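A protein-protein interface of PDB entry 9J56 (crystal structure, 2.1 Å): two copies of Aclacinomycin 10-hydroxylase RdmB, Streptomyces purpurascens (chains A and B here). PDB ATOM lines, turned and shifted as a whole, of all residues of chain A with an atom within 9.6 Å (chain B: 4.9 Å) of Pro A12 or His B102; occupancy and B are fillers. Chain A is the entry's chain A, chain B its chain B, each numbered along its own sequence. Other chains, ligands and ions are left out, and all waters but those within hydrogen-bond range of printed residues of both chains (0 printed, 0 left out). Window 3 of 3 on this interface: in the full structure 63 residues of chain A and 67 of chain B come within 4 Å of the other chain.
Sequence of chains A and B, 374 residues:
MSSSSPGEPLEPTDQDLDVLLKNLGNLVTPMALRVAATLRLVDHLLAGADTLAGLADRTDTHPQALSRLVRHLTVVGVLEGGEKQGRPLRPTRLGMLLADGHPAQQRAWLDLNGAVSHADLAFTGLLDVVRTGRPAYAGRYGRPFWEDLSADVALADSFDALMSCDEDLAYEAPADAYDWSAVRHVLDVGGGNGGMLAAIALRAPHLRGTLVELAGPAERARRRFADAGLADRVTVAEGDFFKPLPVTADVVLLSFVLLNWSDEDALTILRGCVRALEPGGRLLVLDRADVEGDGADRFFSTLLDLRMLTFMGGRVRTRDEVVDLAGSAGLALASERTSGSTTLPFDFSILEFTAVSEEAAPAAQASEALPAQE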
ATOM      1  N   GLU A  11      24.288  -3.384  -0.476  1.00  0.00           N
ATOM      2  CA  GLU A  11      25.252  -2.280  -0.538  1.00  0.00           C
ATOM      3  C   GLU A  11      25.241  -1.234   0.611  1.00  0.00           C
ATOM      4  O   GLU A  11      25.358  -0.042   0.329  1.00  0.00           O
ATOM      5  CB  GLU A  11      25.041  -1.530  -1.856  1.00  0.00           C
ATOM      6  N   PRO A  12      25.138  -1.649   1.880  1.00  0.00           N
ATOM      7  CA  PRO A  12      24.959  -0.660   2.965  1.00  0.00           C
ATOM      8  C   PRO A  12      26.203   0.187   3.216  1.00  0.00           C
ATOM      9  O   PRO A  12      27.308  -0.333   3.371  1.00  0.00           O
ATOM     10  CB  PRO A  12      24.623  -1.524   4.188  1.00  0.00           C
ATOM     11  CG  PRO A  12      24.285  -2.868   3.649  1.00  0.00           C
ATOM     12  CD  PRO A  12      25.089  -3.024   2.403  1.00  0.00           C
ATOM     13  N   THR A  13      26.004   1.506   3.299  1.00  0.00           N
ATOM     14  CA  THR A  13      27.091   2.448   3.533  1.00  0.00           C
ATOM     15  C   THR A  13      27.434   2.509   5.020  1.00  0.00           C
ATOM     16  O   THR A  13      26.808   1.853   5.858  1.00  0.00           O
ATOM     17  CB  THR A  13      26.727   3.837   3.007  1.00  0.00           C
ATOM     18  OG1 THR A  13      25.711   4.418   3.837  1.00  0.00           O
ATOM     19  CG2 THR A  13      26.221   3.763   1.568  1.00  0.00           C
ATOM     20  N   ASP A  14      28.454   3.306   5.356  1.00  0.00           N
ATOM     21  CA  ASP A  14      28.817   3.479   6.759  1.00  0.00           C
ATOM     22  C   ASP A  14      27.757   4.283   7.496  1.00  0.00           C
ATOM     23  O   ASP A  14      27.463   4.007   8.664  1.00  0.00           O
ATOM     24  CB  ASP A  14      30.180   4.160   6.882  1.00  0.00           C
ATOM     25  N   GLN A  15      27.181   5.286   6.826  1.00  0.00           N
ATOM     26  CA  GLN A  15      26.123   6.084   7.435  1.00  0.00           C
ATOM     27  C   GLN A  15      24.899   5.229   7.737  1.00  0.00           C
ATOM     28  O   GLN A  15      24.222   5.435   8.754  1.00  0.00           O
ATOM     29  CB  GLN A  15      25.754   7.255   6.521  1.00  0.00           C
ATOM     30  N   ASP A  16      24.600   4.264   6.863  1.00  0.00           N
ATOM     31  CA  ASP A  16      23.496   3.341   7.108  1.00  0.00           C
ATOM     32  C   ASP A  16      23.650   2.643   8.452  1.00  0.00           C
ATOM     33  O   ASP A  16      22.703   2.583   9.246  1.00  0.00           O
ATOM     34  CB  ASP A  16      23.412   2.311   5.983  1.00  0.00           C
ATOM     35  CG  ASP A  16      23.063   2.933   4.650  1.00  0.00           C
ATOM     36  OD1 ASP A  16      22.578   4.091   4.627  1.00  0.00           O
ATOM     37  OD2 ASP A  16      23.285   2.266   3.618  1.00  0.00           O
ATOM     38  N   LEU A  17      24.843   2.105   8.729  1.00  0.00           N
ATOM     39  CA  LEU A  17      25.045   1.400   9.990  1.00  0.00           C
ATOM     40  C   LEU A  17      24.939   2.351  11.173  1.00  0.00           C
ATOM     41  O   LEU A  17      24.417   1.981  12.230  1.00  0.00           O
ATOM     42  CB  LEU A  17      26.399   0.683   9.996  1.00  0.00           C
ATOM     43  CG  LEU A  17      26.682  -0.217  11.205  1.00  0.00           C
ATOM     44  CD1 LEU A  17      25.501  -1.123  11.520  1.00  0.00           C
ATOM     45  CD2 LEU A  17      27.948  -1.040  11.005  1.00  0.00           C
ATOM     46  N   ASP A  18      25.455   3.570  11.022  1.00  0.00           N
ATOM     47  CA  ASP A  18      25.274   4.585  12.056  1.00  0.00           C
ATOM     48  C   ASP A  18      23.795   4.807  12.360  1.00  0.00           C
ATOM     49  O   ASP A  18      23.403   4.934  13.527  1.00  0.00           O
ATOM     50  CB  ASP A  18      25.938   5.890  11.617  1.00  0.00           C
ATOM     51  CG  ASP A  18      26.020   6.913  12.736  1.00  0.00           C
ATOM     52  OD1 ASP A  18      26.759   6.671  13.716  1.00  0.00           O
ATOM     53  OD2 ASP A  18      25.339   7.964  12.632  1.00  0.00           O
ATOM     54  N   LEU A  20      21.252   2.683  11.918  1.00  0.00           N
ATOM     55  CA  LEU A  20      20.640   1.532  12.577  1.00  0.00           C
ATOM     56  C   LEU A  20      21.026   1.454  14.047  1.00  0.00           C
ATOM     57  O   LEU A  20      20.181   1.149  14.898  1.00  0.00           O
ATOM     58  CB  LEU A  20      21.025   0.240  11.851  1.00  0.00           C
ATOM     59  CG  LEU A  20      20.286  -0.982  12.391  1.00  0.00           C
ATOM     60  CD1 LEU A  20      18.912  -1.049  11.766  1.00  0.00           C
ATOM     61  CD2 LEU A  20      21.061  -2.272  12.099  1.00  0.00           C
ATOM     62  N   LEU A  21      22.289   1.745  14.366  1.00  0.00           N
ATOM     63  CA  LEU A  21      22.785   1.568  15.729  1.00  0.00           C
ATOM     64  C   LEU A  21      22.308   2.672  16.663  1.00  0.00           C
ATOM     65  O   LEU A  21      22.001   2.414  17.835  1.00  0.00           O
ATOM     66  CB  LEU A  21      24.316   1.518  15.726  1.00  0.00           C
ATOM     67  CG  LEU A  21      24.965   0.269  15.126  1.00  0.00           C
ATOM     68  CD1 LEU A  21      26.466   0.459  15.011  1.00  0.00           C
ATOM     69  CD2 LEU A  21      24.653  -0.957  15.970  1.00  0.00           C
ATOM     70  N   ARG B  93      19.002  -0.173   0.740  1.00  0.00           N
ATOM     71  CA  ARG B  93      20.432  -0.251   1.036  1.00  0.00           C
ATOM     72  C   ARG B  93      20.663  -0.404   2.531  1.00  0.00           C
ATOM     73  O   ARG B  93      21.577  -1.117   2.953  1.00  0.00           O
ATOM     74  CB  ARG B  93      21.162   0.987   0.507  1.00  0.00           C
ATOM     75  N   MET B  96      19.702  -3.949   3.900  1.00  0.00           N
ATOM     76  CA  MET B  96      20.689  -5.001   3.698  1.00  0.00           C
ATOM     77  C   MET B  96      21.595  -5.190   4.894  1.00  0.00           C
ATOM     78  O   MET B  96      22.553  -5.970   4.854  1.00  0.00           O
ATOM     79  CB  MET B  96      21.521  -4.724   2.445  1.00  0.00           C
ATOM     80  CG  MET B  96      20.713  -4.799   1.163  1.00  0.00           C
ATOM     81  SD  MET B  96      20.755  -6.434   0.412  1.00  0.00           S
ATOM     82  CE  MET B  96      19.440  -7.256   1.326  1.00  0.00           C
ATOM     83  N   LEU B  97      21.338  -4.499   5.999  1.00  0.00           N
ATOM     84  CA  LEU B  97      22.050  -4.795   7.230  1.00  0.00           C
ATOM     85  C   LEU B  97      21.443  -5.979   7.966  1.00  0.00           C
ATOM     86  O   LEU B  97      22.123  -6.597   8.790  1.00  0.00           O
ATOM     87  CB  LEU B  97      22.068  -3.558   8.126  1.00  0.00           C
ATOM     88  CG  LEU B  97      22.963  -2.420   7.634  1.00  0.00           C
ATOM     89  CD1 LEU B  97      22.968  -1.280   8.647  1.00  0.00           C
ATOM     90  CD2 LEU B  97      24.375  -2.926   7.417  1.00  0.00           C
ATOM     91  N   ALA B  99      20.491  -8.635   6.323  1.00  0.00           N
ATOM     92  CA  ALA B  99      20.883  -9.814   5.564  1.00  0.00           C
ATOM     93  C   ALA B  99      21.858 -10.636   6.390  1.00  0.00           C
ATOM     94  O   ALA B  99      22.836 -10.101   6.922  1.00  0.00           O
ATOM     95  CB  ALA B  99      21.527  -9.416   4.234  1.00  0.00           C
ATOM     96  N   ASP B 100      21.597 -11.938   6.508  1.00  0.00           N
ATOM     97  CA  ASP B 100      22.453 -12.747   7.370  1.00  0.00           C
ATOM     98  C   ASP B 100      23.911 -12.741   6.926  1.00  0.00           C
ATOM     99  O   ASP B 100      24.787 -13.059   7.735  1.00  0.00           O
ATOM    100  CB  ASP B 100      21.956 -14.188   7.449  1.00  0.00           C
ATOM    101  CG  ASP B 100      22.078 -14.754   8.850  1.00  0.00           C
ATOM    102  OD1 ASP B 100      22.838 -14.165   9.652  1.00  0.00           O
ATOM    103  OD2 ASP B 100      21.400 -15.761   9.157  1.00  0.00           O
ATOM    104  N   GLY B 101      24.196 -12.357   5.681  1.00  0.00           N
ATOM    105  CA  GLY B 101      25.566 -12.345   5.204  1.00  0.00           C
ATOM    106  C   GLY B 101      26.379 -11.102   5.524  1.00  0.00           C
ATOM    107  O   GLY B 101      27.597 -11.121   5.327  1.00  0.00           O
ATOM    108  N   HIS B 102      25.756 -10.032   6.018  1.00  0.00           N
ATOM    109  CA  HIS B 102      26.485  -8.778   6.165  1.00  0.00           C
ATOM    110  C   HIS B 102      27.510  -8.882   7.294  1.00  0.00           C
ATOM    111  O   HIS B 102      27.214  -9.449   8.350  1.00  0.00           O
ATOM    112  CB  HIS B 102      25.544  -7.596   6.431  1.00  0.00           C
ATOM    113  CG  HIS B 102      26.231  -6.271   6.332  1.00  0.00           C
ATOM    114  ND1 HIS B 102      26.788  -5.636   7.422  1.00  0.00           N
ATOM    115  CD2 HIS B 102      26.514  -5.493   5.259  1.00  0.00           C
ATOM    116  CE1 HIS B 102      27.362  -4.512   7.029  1.00  0.00           C
ATOM    117  NE2 HIS B 102      27.208  -4.401   5.720  1.00  0.00           N
ATOM    118  N   PRO B 103      28.720  -8.339   7.098  1.00  0.00           N
ATOM    119  CA  PRO B 103      29.774  -8.502   8.117  1.00  0.00           C
ATOM    120  C   PRO B 103      29.417  -7.951   9.490  1.00  0.00           C
ATOM    121  O   PRO B 103      29.825  -8.538  10.501  1.00  0.00           O
ATOM    122  CB  PRO B 103      30.975  -7.761   7.502  1.00  0.00           C
ATOM    123  CG  PRO B 103      30.446  -7.046   6.273  1.00  0.00           C
ATOM    124  CD  PRO B 103      29.253  -7.812   5.829  1.00  0.00           C
ATOM    125  N   ALA B 104      28.663  -6.846   9.569  1.00  0.00           N
ATOM    126  CA  ALA B 104      28.357  -6.285  10.880  1.00  0.00           C
ATOM    127  C   ALA B 104      27.378  -7.141  11.674  1.00  0.00           C
ATOM    128  O   ALA B 104      27.140  -6.843  12.850  1.00  0.00           O
ATOM    129  CB  ALA B 104      27.817  -4.860  10.739  1.00  0.00           C
ATOM    130  N   GLN B 105      26.794  -8.173  11.059  1.00  0.00           N
ATOM    131  CA  GLN B 105      26.007  -9.190  11.763  1.00  0.00           C
ATOM    132  C   GLN B 105      24.867  -8.592  12.595  1.00  0.00           C
ATOM    133  O   GLN B 105      24.502  -9.129  13.644  1.00  0.00           O
ATOM    134  CB  GLN B 105      26.914 -10.061  12.644  1.00  0.00           C
ATOM    135  CG  GLN B 105      27.829 -10.982  11.834  1.00  0.00           C
ATOM    136  CD  GLN B 105      27.041 -12.015  11.060  1.00  0.00           C
ATOM    137  OE1 GLN B 105      26.634 -13.039  11.610  1.00  0.00           O
ATOM    138  NE2 GLN B 105      26.815 -11.755   9.780  1.00  0.00           N
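ND1 of His B102 lies within hydrogen-bond range of N of Ala B104 (3.1 Å). O of His B102 is in hydrogen-bond range of NE2 of Gln B105. N of Thr A13 sits at hydrogen-bond distance from OD2 of Asp A16 (2.8 Å).
Among the printed residues, pairs that only touch across the chains: Pro A12 with Arg B93 (3.3 Å), Pro A12 with Met B96 (3.5 Å), Pro A12 with Leu B97 (3.5 Å), Pro A12 with His B102 (3.8 Å), Asp A16 with Arg B93 (3.8 Å), Asp A16 with Leu B97 (3.9 Å), Leu A17 with Leu B97 (3.6 Å) and Leu A17 with Ala B104 (3.8 Å).
Pro A12 touches four residues of chain B. Printed residues of chain B within 4 Å of Asp A16: Arg B93 (3.8 Å) and Leu B97 (3.9 Å). Of the printed residues of chain B, Leu A17 touches Leu B97 (3.6 Å) and Ala B104 (3.8 Å). Printed residues of chain A within 4 Å of Arg B93: Pro A12 (3.3 Å) and Asp A16 (3.8 Å). Printed residues of chain A within 4 Å of Met B96: Pro A12 (3.5 Å). No residue of chain A comes within 4 Å of Ala B99. No residue of chain A comes within 4 Å of Gly B101. Of chain A, only Pro A12 comes within 4 Å of His B102. No residue of chain A comes within 4 Å of Pro B103.
Hydrophobic or aromatic side chains of chain A within 4 Å of the printed part of chain B: Pro A12 and Leu A17. Hydrophobic or aromatic side chains of chain B within 4 Å of the printed part of chain A: Met B96, Leu B97, His B102 and Ala B104. Among the printed residues, no Asp or Glu carboxylate lies within 4 Å of a Lys or Arg side-chain nitrogen of the other chain.
No position is printed for both chains.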
